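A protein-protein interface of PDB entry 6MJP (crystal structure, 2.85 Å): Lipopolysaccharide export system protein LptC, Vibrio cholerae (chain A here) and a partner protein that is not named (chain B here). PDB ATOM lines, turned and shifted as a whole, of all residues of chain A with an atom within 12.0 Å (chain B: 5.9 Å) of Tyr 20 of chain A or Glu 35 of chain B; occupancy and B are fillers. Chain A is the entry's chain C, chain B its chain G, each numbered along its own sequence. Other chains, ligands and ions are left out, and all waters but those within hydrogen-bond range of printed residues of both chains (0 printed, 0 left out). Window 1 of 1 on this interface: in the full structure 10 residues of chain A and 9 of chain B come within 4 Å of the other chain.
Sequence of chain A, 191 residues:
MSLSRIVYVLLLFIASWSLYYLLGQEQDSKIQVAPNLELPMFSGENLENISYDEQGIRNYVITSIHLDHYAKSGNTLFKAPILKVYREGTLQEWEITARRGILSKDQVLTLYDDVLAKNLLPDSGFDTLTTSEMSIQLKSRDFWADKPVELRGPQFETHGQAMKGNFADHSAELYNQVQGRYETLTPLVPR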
ATOM      1  N   VAL A   9     -22.385 -24.767   3.465  1.00  0.00           N
ATOM      2  CA  VAL A   9     -22.885 -23.738   4.380  1.00  0.00           C
ATOM      3  C   VAL A   9     -21.798 -23.302   5.363  1.00  0.00           C
ATOM      4  O   VAL A   9     -21.605 -22.102   5.590  1.00  0.00           O
ATOM      5  CB  VAL A   9     -24.153 -24.215   5.112  1.00  0.00           C
ATOM      6  CG1 VAL A   9     -24.513 -23.246   6.198  1.00  0.00           C
ATOM      7  CG2 VAL A   9     -25.309 -24.303   4.160  1.00  0.00           C
ATOM      8  N   LEU A  11     -18.642 -23.334   4.791  1.00  0.00           N
ATOM      9  CA  LEU A  11     -17.748 -22.490   3.998  1.00  0.00           C
ATOM     10  C   LEU A  11     -18.332 -21.095   3.800  1.00  0.00           C
ATOM     11  O   LEU A  11     -17.598 -20.101   3.787  1.00  0.00           O
ATOM     12  CB  LEU A  11     -17.470 -23.137   2.647  1.00  0.00           C
ATOM     13  CG  LEU A  11     -16.608 -24.395   2.617  1.00  0.00           C
ATOM     14  CD1 LEU A  11     -16.631 -25.019   1.246  1.00  0.00           C
ATOM     15  CD2 LEU A  11     -15.187 -24.063   2.984  1.00  0.00           C
ATOM     16  N   LEU A  12     -19.647 -20.993   3.656  1.00  0.00           N
ATOM     17  CA  LEU A  12     -20.227 -19.675   3.463  1.00  0.00           C
ATOM     18  C   LEU A  12     -20.153 -18.863   4.745  1.00  0.00           C
ATOM     19  O   LEU A  12     -20.000 -17.636   4.707  1.00  0.00           O
ATOM     20  CB  LEU A  12     -21.662 -19.814   2.973  1.00  0.00           C
ATOM     21  CG  LEU A  12     -22.349 -18.572   2.435  1.00  0.00           C
ATOM     22  CD1 LEU A  12     -21.435 -17.800   1.497  1.00  0.00           C
ATOM     23  CD2 LEU A  12     -23.560 -19.081   1.715  1.00  0.00           C
ATOM     24  N   PHE A  13     -20.249 -19.538   5.895  1.00  0.00           N
ATOM     25  CA  PHE A  13     -20.068 -18.874   7.186  1.00  0.00           C
ATOM     26  C   PHE A  13     -18.683 -18.250   7.297  1.00  0.00           C
ATOM     27  O   PHE A  13     -18.543 -17.067   7.624  1.00  0.00           O
ATOM     28  CB  PHE A  13     -20.272 -19.879   8.324  1.00  0.00           C
ATOM     29  CG  PHE A  13     -21.714 -20.177   8.647  1.00  0.00           C
ATOM     30  CD1 PHE A  13     -22.711 -19.253   8.404  1.00  0.00           C
ATOM     31  CD2 PHE A  13     -22.062 -21.395   9.216  1.00  0.00           C
ATOM     32  CE1 PHE A  13     -24.037 -19.538   8.715  1.00  0.00           C
ATOM     33  CE2 PHE A  13     -23.378 -21.686   9.530  1.00  0.00           C
ATOM     34  CZ  PHE A  13     -24.369 -20.754   9.278  1.00  0.00           C
ATOM     35  N   ILE A  14     -17.643 -19.049   7.037  1.00  0.00           N
ATOM     36  CA  ILE A  14     -16.271 -18.565   7.132  1.00  0.00           C
ATOM     37  C   ILE A  14     -16.029 -17.423   6.157  1.00  0.00           C
ATOM     38  O   ILE A  14     -15.325 -16.458   6.476  1.00  0.00           O
ATOM     39  CB  ILE A  14     -15.278 -19.705   6.868  1.00  0.00           C
ATOM     40  CG1 ILE A  14     -15.537 -20.936   7.742  1.00  0.00           C
ATOM     41  CG2 ILE A  14     -13.851 -19.195   7.003  1.00  0.00           C
ATOM     42  CD1 ILE A  14     -14.762 -22.153   7.251  1.00  0.00           C
ATOM     43  N   ALA A  15     -16.572 -17.526   4.940  1.00  0.00           N
ATOM     44  CA  ALA A  15     -16.370 -16.470   3.948  1.00  0.00           C
ATOM     45  C   ALA A  15     -16.998 -15.159   4.403  1.00  0.00           C
ATOM     46  O   ALA A  15     -16.333 -14.116   4.417  1.00  0.00           O
ATOM     47  CB  ALA A  15     -16.933 -16.891   2.595  1.00  0.00           C
ATOM     48  N   SER A  16     -18.282 -15.194   4.780  1.00  0.00           N
ATOM     49  CA  SER A  16     -18.936 -14.003   5.312  1.00  0.00           C
ATOM     50  C   SER A  16     -18.160 -13.419   6.484  1.00  0.00           C
ATOM     51  O   SER A  16     -17.964 -12.198   6.562  1.00  0.00           O
ATOM     52  CB  SER A  16     -20.358 -14.327   5.755  1.00  0.00           C
ATOM     53  OG  SER A  16     -21.183 -14.707   4.672  1.00  0.00           O
ATOM     54  N   TRP A  17     -17.717 -14.276   7.414  1.00  0.00           N
ATOM     55  CA  TRP A  17     -17.014 -13.785   8.594  1.00  0.00           C
ATOM     56  C   TRP A  17     -15.707 -13.097   8.213  1.00  0.00           C
ATOM     57  O   TRP A  17     -15.438 -11.981   8.670  1.00  0.00           O
ATOM     58  CB  TRP A  17     -16.764 -14.918   9.592  1.00  0.00           C
ATOM     59  CG  TRP A  17     -16.200 -14.378  10.872  1.00  0.00           C
ATOM     60  CD1 TRP A  17     -16.898 -13.951  11.971  1.00  0.00           C
ATOM     61  CD2 TRP A  17     -14.819 -14.138  11.160  1.00  0.00           C
ATOM     62  NE1 TRP A  17     -16.030 -13.476  12.925  1.00  0.00           N
ATOM     63  CE2 TRP A  17     -14.748 -13.579  12.452  1.00  0.00           C
ATOM     64  CE3 TRP A  17     -13.633 -14.352  10.451  1.00  0.00           C
ATOM     65  CZ2 TRP A  17     -13.537 -13.235  13.047  1.00  0.00           C
ATOM     66  CZ3 TRP A  17     -12.437 -14.008  11.041  1.00  0.00           C
ATOM     67  CH2 TRP A  17     -12.395 -13.456  12.327  1.00  0.00           C
ATOM     68  N   SER A  18     -14.891 -13.731   7.361  1.00  0.00           N
ATOM     69  CA  SER A  18     -13.657 -13.088   6.906  1.00  0.00           C
ATOM     70  C   SER A  18     -13.932 -11.759   6.202  1.00  0.00           C
ATOM     71  O   SER A  18     -13.196 -10.786   6.403  1.00  0.00           O
ATOM     72  CB  SER A  18     -12.870 -14.003   5.966  1.00  0.00           C
ATOM     73  OG  SER A  18     -12.559 -15.249   6.549  1.00  0.00           O
ATOM     74  N   LEU A  19     -14.951 -11.702   5.339  1.00  0.00           N
ATOM     75  CA  LEU A  19     -15.185 -10.459   4.609  1.00  0.00           C
ATOM     76  C   LEU A  19     -15.514  -9.335   5.574  1.00  0.00           C
ATOM     77  O   LEU A  19     -14.922  -8.249   5.513  1.00  0.00           O
ATOM     78  CB  LEU A  19     -16.305 -10.625   3.577  1.00  0.00           C
ATOM     79  CG  LEU A  19     -16.802  -9.305   2.943  1.00  0.00           C
ATOM     80  CD1 LEU A  19     -15.749  -8.622   2.069  1.00  0.00           C
ATOM     81  CD2 LEU A  19     -18.083  -9.497   2.157  1.00  0.00           C
ATOM     82  N   TYR A  20     -16.429  -9.603   6.508  1.00  0.00           N
ATOM     83  CA  TYR A  20     -16.877  -8.578   7.441  1.00  0.00           C
ATOM     84  C   TYR A  20     -15.820  -8.259   8.494  1.00  0.00           C
ATOM     85  O   TYR A  20     -15.798  -7.144   9.022  1.00  0.00           O
ATOM     86  CB  TYR A  20     -18.194  -9.007   8.075  1.00  0.00           C
ATOM     87  CG  TYR A  20     -19.363  -8.838   7.133  1.00  0.00           C
ATOM     88  CD1 TYR A  20     -19.740  -7.574   6.698  1.00  0.00           C
ATOM     89  CD2 TYR A  20     -20.088  -9.929   6.670  1.00  0.00           C
ATOM     90  CE1 TYR A  20     -20.806  -7.396   5.836  1.00  0.00           C
ATOM     91  CE2 TYR A  20     -21.167  -9.762   5.796  1.00  0.00           C
ATOM     92  CZ  TYR A  20     -21.518  -8.490   5.386  1.00  0.00           C
ATOM     93  OH  TYR A  20     -22.578  -8.300   4.526  1.00  0.00           O
ATOM     94  N   TYR A  21     -14.945  -9.215   8.818  1.00  0.00           N
ATOM     95  CA  TYR A  21     -13.789  -8.881   9.639  1.00  0.00           C
ATOM     96  C   TYR A  21     -12.869  -7.911   8.909  1.00  0.00           C
ATOM     97  O   TYR A  21     -12.379  -6.947   9.506  1.00  0.00           O
ATOM     98  CB  TYR A  21     -13.032 -10.147  10.042  1.00  0.00           C
ATOM     99  CG  TYR A  21     -11.780  -9.868  10.840  1.00  0.00           C
ATOM    100  CD1 TYR A  21     -11.846  -9.582  12.199  1.00  0.00           C
ATOM    101  CD2 TYR A  21     -10.530  -9.872  10.233  1.00  0.00           C
ATOM    102  CE1 TYR A  21     -10.700  -9.317  12.930  1.00  0.00           C
ATOM    103  CE2 TYR A  21      -9.376  -9.607  10.960  1.00  0.00           C
ATOM    104  CZ  TYR A  21      -9.467  -9.332  12.303  1.00  0.00           C
ATOM    105  OH  TYR A  21      -8.318  -9.068  13.017  1.00  0.00           O
ATOM    106  N   LEU A  22     -12.644  -8.131   7.612  1.00  0.00           N
ATOM    107  CA  LEU A  22     -11.823  -7.207   6.833  1.00  0.00           C
ATOM    108  C   LEU A  22     -12.463  -5.829   6.741  1.00  0.00           C
ATOM    109  O   LEU A  22     -11.760  -4.811   6.773  1.00  0.00           O
ATOM    110  CB  LEU A  22     -11.577  -7.768   5.433  1.00  0.00           C
ATOM    111  CG  LEU A  22     -10.520  -8.863   5.245  1.00  0.00           C
ATOM    112  CD1 LEU A  22     -10.514  -9.286   3.801  1.00  0.00           C
ATOM    113  CD2 LEU A  22      -9.124  -8.412   5.669  1.00  0.00           C
ATOM    114  N   LEU A  23     -13.793  -5.777   6.607  1.00  0.00           N
ATOM    115  CA  LEU A  23     -14.481  -4.489   6.602  1.00  0.00           C
ATOM    116  C   LEU A  23     -14.367  -3.796   7.950  1.00  0.00           C
ATOM    117  O   LEU A  23     -14.148  -2.581   8.016  1.00  0.00           O
ATOM    118  CB  LEU A  23     -15.950  -4.671   6.233  1.00  0.00           C
ATOM    119  CG  LEU A  23     -16.199  -5.220   4.833  1.00  0.00           C
ATOM    120  CD1 LEU A  23     -17.684  -5.241   4.531  1.00  0.00           C
ATOM    121  CD2 LEU A  23     -15.440  -4.395   3.809  1.00  0.00           C
ATOM    122  N   GLY A  24     -14.528  -4.551   9.039  1.00  0.00           N
ATOM    123  CA  GLY A  24     -14.357  -3.977  10.361  1.00  0.00           C
ATOM    124  C   GLY A  24     -12.948  -3.493  10.616  1.00  0.00           C
ATOM    125  O   GLY A  24     -12.753  -2.460  11.259  1.00  0.00           O
ATOM    126  N   GLN A  25     -11.949  -4.218  10.112  1.00  0.00           N
ATOM    127  CA  GLN A  25     -10.567  -3.784  10.288  1.00  0.00           C
ATOM    128  C   GLN A  25     -10.312  -2.455   9.584  1.00  0.00           C
ATOM    129  O   GLN A  25      -9.673  -1.559  10.149  1.00  0.00           O
ATOM    130  CB  GLN A  25      -9.602  -4.853   9.779  1.00  0.00           C
ATOM    131  CG  GLN A  25      -9.595  -6.135  10.587  1.00  0.00           C
ATOM    132  CD  GLN A  25      -9.237  -5.932  12.049  1.00  0.00           C
ATOM    133  OE1 GLN A  25     -10.105  -5.674  12.888  1.00  0.00           O
ATOM    134  NE2 GLN A  25      -7.954  -6.066  12.367  1.00  0.00           N
ATOM    135  N   GLU A  26     -10.785  -2.308   8.343  1.00  0.00           N
ATOM    136  CA  GLU A  26     -10.567  -1.044   7.651  1.00  0.00           C
ATOM    137  C   GLU A  26     -11.440   0.054   8.237  1.00  0.00           C
ATOM    138  O   GLU A  26     -11.129   1.242   8.084  1.00  0.00           O
ATOM    139  CB  GLU A  26     -10.818  -1.184   6.152  1.00  0.00           C
ATOM    140  CG  GLU A  26     -12.278  -1.350   5.763  1.00  0.00           C
ATOM    141  CD  GLU A  26     -12.479  -1.388   4.257  1.00  0.00           C
ATOM    142  OE1 GLU A  26     -11.482  -1.211   3.523  1.00  0.00           O
ATOM    143  OE2 GLU A  26     -13.627  -1.595   3.805  1.00  0.00           O
ATOM    144  N   GLN A  27     -12.530  -0.323   8.909  1.00  0.00           N
ATOM    145  CA  GLN A  27     -13.341   0.658   9.620  1.00  0.00           C
ATOM    146  C   GLN A  27     -12.591   1.212  10.826  1.00  0.00           C
ATOM    147  O   GLN A  27     -12.469   2.431  10.984  1.00  0.00           O
ATOM    148  CB  GLN A  27     -14.668   0.028  10.044  1.00  0.00           C
ATOM    149  CG  GLN A  27     -15.551   0.953  10.863  1.00  0.00           C
ATOM    150  CD  GLN A  27     -16.656   0.218  11.601  1.00  0.00           C
ATOM    151  OE1 GLN A  27     -16.655  -1.011  11.685  1.00  0.00           O
ATOM    152  NE2 GLN A  27     -17.608   0.973  12.144  1.00  0.00           N
ATOM    153  N   ASP A  28     -12.064   0.326  11.680  1.00  0.00           N
ATOM    154  CA  ASP A  28     -11.246   0.771  12.807  1.00  0.00           C
ATOM    155  C   ASP A  28     -10.030   1.561  12.343  1.00  0.00           C
ATOM    156  O   ASP A  28      -9.578   2.473  13.044  1.00  0.00           O
ATOM    157  CB  ASP A  28     -10.804  -0.424  13.651  1.00  0.00           C
ATOM    158  CG  ASP A  28     -11.964  -1.094  14.360  1.00  0.00           C
ATOM    159  OD1 ASP A  28     -13.098  -0.591  14.224  1.00  0.00           O
ATOM    160  OD2 ASP A  28     -11.750  -2.118  15.049  1.00  0.00           O
ATOM    161  N   SER A  29      -9.490   1.234  11.167  1.00  0.00           N
ATOM    162  CA  SER A  29      -8.410   2.041  10.613  1.00  0.00           C
ATOM    163  C   SER A  29      -8.913   3.410  10.188  1.00  0.00           C
ATOM    164  O   SER A  29      -8.148   4.381  10.190  1.00  0.00           O
ATOM    165  CB  SER A  29      -7.766   1.324   9.427  1.00  0.00           C
ATOM    166  OG  SER A  29      -8.605   1.368   8.282  1.00  0.00           O
ATOM    167  N   ILE B  30     -28.139 -15.961   5.210  1.00  0.00           N
ATOM    168  CA  ILE B  30     -27.089 -16.435   6.107  1.00  0.00           C
ATOM    169  C   ILE B  30     -25.896 -15.493   6.081  1.00  0.00           C
ATOM    170  O   ILE B  30     -25.165 -15.376   7.077  1.00  0.00           O
ATOM    171  CB  ILE B  30     -26.673 -17.884   5.785  1.00  0.00           C
ATOM    172  CG1 ILE B  30     -26.248 -18.047   4.338  1.00  0.00           C
ATOM    173  CG2 ILE B  30     -27.816 -18.840   6.006  1.00  0.00           C
ATOM    174  CD1 ILE B  30     -26.246 -19.511   3.914  1.00  0.00           C
ATOM    175  N   ILE B  31     -25.677 -14.805   4.963  1.00  0.00           N
ATOM    176  CA  ILE B  31     -24.653 -13.768   4.942  1.00  0.00           C
ATOM    177  C   ILE B  31     -25.061 -12.601   5.842  1.00  0.00           C
ATOM    178  O   ILE B  31     -24.245 -12.095   6.620  1.00  0.00           O
ATOM    179  CB  ILE B  31     -24.377 -13.318   3.495  1.00  0.00           C
ATOM    180  CG1 ILE B  31     -23.834 -14.480   2.654  1.00  0.00           C
ATOM    181  CG2 ILE B  31     -23.369 -12.182   3.464  1.00  0.00           C
ATOM    182  CD1 ILE B  31     -23.440 -14.088   1.239  1.00  0.00           C
ATOM    183  N   LYS B  32     -26.332 -12.172   5.772  1.00  0.00           N
ATOM    184  CA  LYS B  32     -26.812 -11.128   6.681  1.00  0.00           C
ATOM    185  C   LYS B  32     -26.651 -11.550   8.143  1.00  0.00           C
ATOM    186  O   LYS B  32     -26.274 -10.732   8.995  1.00  0.00           O
ATOM    187  CB  LYS B  32     -28.279 -10.789   6.391  1.00  0.00           C
ATOM    188  CG  LYS B  32     -28.534  -9.631   5.411  1.00  0.00           C
ATOM    189  CD  LYS B  32     -30.031  -9.494   5.091  1.00  0.00           C
ATOM    190  CE  LYS B  32     -30.295  -8.354   4.137  1.00  0.00           C
ATOM    191  NZ  LYS B  32     -29.638  -7.125   4.655  1.00  0.00           N
ATOM    192  N   TYR B  33     -26.913 -12.829   8.450  1.00  0.00           N
ATOM    193  CA  TYR B  33     -26.812 -13.290   9.835  1.00  0.00           C
ATOM    194  C   TYR B  33     -25.382 -13.209  10.365  1.00  0.00           C
ATOM    195  O   TYR B  33     -25.175 -12.932  11.554  1.00  0.00           O
ATOM    196  CB  TYR B  33     -27.352 -14.713  10.005  1.00  0.00           C
ATOM    197  CG  TYR B  33     -27.582 -15.035  11.460  1.00  0.00           C
ATOM    198  CD1 TYR B  33     -26.567 -15.564  12.248  1.00  0.00           C
ATOM    199  CD2 TYR B  33     -28.798 -14.751  12.065  1.00  0.00           C
ATOM    200  CE1 TYR B  33     -26.765 -15.827  13.602  1.00  0.00           C
ATOM    201  CE2 TYR B  33     -29.011 -15.010  13.417  1.00  0.00           C
ATOM    202  CZ  TYR B  33     -27.990 -15.550  14.176  1.00  0.00           C
ATOM    203  OH  TYR B  33     -28.198 -15.813  15.504  1.00  0.00           O
ATOM    204  N   VAL B  34     -24.383 -13.471   9.523  1.00  0.00           N
ATOM    205  CA  VAL B  34     -23.008 -13.280   9.975  1.00  0.00           C
ATOM    206  C   VAL B  34     -22.699 -11.795  10.119  1.00  0.00           C
ATOM    207  O   VAL B  34     -21.970 -11.386  11.036  1.00  0.00           O
ATOM    208  CB  VAL B  34     -22.020 -13.987   9.030  1.00  0.00           C
ATOM    209  CG1 VAL B  34     -20.584 -13.804   9.505  1.00  0.00           C
ATOM    210  CG2 VAL B  34     -22.347 -15.468   8.937  1.00  0.00           C
ATOM    211  N   GLU B  35     -23.256 -10.958   9.238  1.00  0.00           N
ATOM    212  CA  GLU B  35     -23.105  -9.520   9.423  1.00  0.00           C
ATOM    213  C   GLU B  35     -23.701  -9.076  10.754  1.00  0.00           C
ATOM    214  O   GLU B  35     -23.112  -8.252  11.459  1.00  0.00           O
ATOM    215  CB  GLU B  35     -23.743  -8.751   8.267  1.00  0.00           C
ATOM    216  CG  GLU B  35     -24.042  -7.289   8.616  1.00  0.00           C
ATOM    217  CD  GLU B  35     -24.089  -6.358   7.419  1.00  0.00           C
ATOM    218  OE1 GLU B  35     -23.069  -5.691   7.146  1.00  0.00           O
ATOM    219  OE2 GLU B  35     -25.145  -6.285   6.756  1.00  0.00           O
ATOM    220  N   GLN B  36     -24.862  -9.623  11.126  1.00  0.00           N
ATOM    221  CA  GLN B  36     -25.440  -9.292  12.425  1.00  0.00           C
ATOM    222  C   GLN B  36     -24.628  -9.888  13.568  1.00  0.00           C
ATOM    223  O   GLN B  36     -24.629  -9.340  14.676  1.00  0.00           O
ATOM    224  CB  GLN B  36     -26.893  -9.763  12.500  1.00  0.00           C
ATOM    225  CG  GLN B  36     -27.778  -9.204  11.391  1.00  0.00           C
ATOM    226  CD  GLN B  36     -27.744  -7.697  11.342  1.00  0.00           C
ATOM    227  OE1 GLN B  36     -28.125  -7.029  12.299  1.00  0.00           O
ATOM    228  NE2 GLN B  36     -27.280  -7.149  10.227  1.00  0.00           N
ATOM    229  N   LEU B  37     -23.911 -10.991  13.323  1.00  0.00           N
ATOM    230  CA  LEU B  37     -23.034 -11.532  14.357  1.00  0.00           C
ATOM    231  C   LEU B  37     -21.878 -10.584  14.635  1.00  0.00           C
ATOM    232  O   LEU B  37     -21.315 -10.590  15.733  1.00  0.00           O
ATOM    233  CB  LEU B  37     -22.477 -12.897  13.941  1.00  0.00           C
ATOM    234  CG  LEU B  37     -23.379 -14.097  14.192  1.00  0.00           C
ATOM    235  CD1 LEU B  37     -22.674 -15.385  13.825  1.00  0.00           C
ATOM    236  CD2 LEU B  37     -23.809 -14.141  15.641  1.00  0.00           C
ATOM    237  N   ARG B  38     -21.505  -9.756  13.649  1.00  0.00           N
ATOM    238  CA  ARG B  38     -20.442  -8.764  13.832  1.00  0.00           C
ATOM    239  C   ARG B  38     -20.687  -7.852  15.034  1.00  0.00           C
ATOM    240  O   ARG B  38     -19.729  -7.409  15.693  1.00  0.00           O
ATOM    241  CB  ARG B  38     -20.309  -7.917  12.552  1.00  0.00           C
ATOM    242  CG  ARG B  38     -19.105  -6.945  12.541  1.00  0.00           C
ATOM    243  CD  ARG B  38     -17.767  -7.655  12.754  1.00  0.00           C
ATOM    244  NE  ARG B  38     -16.668  -6.689  12.756  1.00  0.00           N
ATOM    245  CZ  ARG B  38     -15.442  -6.935  13.209  1.00  0.00           C
ATOM    246  NH1 ARG B  38     -14.513  -5.984  13.171  1.00  0.00           N
ATOM    247  NH2 ARG B  38     -15.141  -8.126  13.707  1.00  0.00           N
ATOM    248  N   LYS B  39     -21.989  -7.630  15.392  1.00  0.00           N
ATOM    249  CA  LYS B  39     -22.385  -6.699  16.467  1.00  0.00           C
ATOM    250  C   LYS B  39     -23.560  -7.274  17.285  1.00  0.00           C
ATOM    251  O   LYS B  39     -24.577  -6.637  17.502  1.00  0.00           O
ATOM    252  CB  LYS B  39     -22.742  -5.348  15.864  1.00  0.00           C
ATOM    253  CG  LYS B  39     -23.813  -5.393  14.727  1.00  0.00           C
ATOM    254  CD  LYS B  39     -23.830  -4.035  13.986  1.00  0.00           C
ATOM    255  CE  LYS B  39     -22.446  -3.647  13.472  1.00  0.00           C
ATOM    256  NZ  LYS B  39     -22.538  -2.693  12.342  1.00  0.00           N
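Of the 10 printed residues of chain B, 5 touch a printed residue of chain A. Hydrophobic or aromatic side chains of chain B within 4 Å of the printed part of chain A: Ile 30, Ile 31 and Val 34.
O of Leu 12 of chain A lies within hydrogen-bond range of OG of Ser 16 of chain A (3.2 Å). OH of Tyr 21 of chain A is in hydrogen-bond range of NE2 of Gln 25 of chain A, 3.1 Å away.
Printed residues of chain B within 4 Å of Phe 13 of chain A: Val 34 (3.8 Å). Of the printed residues of chain B, Ser 16 of chain A touches Ile 31 and Val 34. Tyr 20 of chain A touches just these residues of chain B: Ile 31, Glu 35 and Arg 38. Ser 29 of chain A touches none of the printed residues of chain B. Of chain A, only Tyr 20 (3.1 Å) comes within 4 Å of Glu 35 of chain B. No residue of chain A comes within 4 Å of Gln 36 of chain B. Arg 38 of chain B touches three residues of chain A. No residue of chain A comes within 4 Å of Lys 39 of chain B.
Among the printed residues, merely in contact across the chains: Tyr 20 of chain A with Glu 35 of chain B (3.1 Å), Ser 16 of chain A with Ile 31 of chain B (3.3 Å), Gly 24 of chain A with Arg 38 of chain B (3.5 Å), Leu 12 of chain A with Ile 30 of chain B (3.5 Å), Trp 17 of chain A with Val 34 of chain B (3.6 Å), Ser 16 of chain A with Val 34 of chain B (3.7 Å), Phe 13 of chain A with Val 34 of chain B (3.8 Å), Tyr 20 of chain A with Arg 38 of chain B (3.9 Å), Tyr 21 of chain A with Arg 38 of chain B (3.9 Å) and Tyr 20 of chain A with Ile 31 of chain B (3.9 Å).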
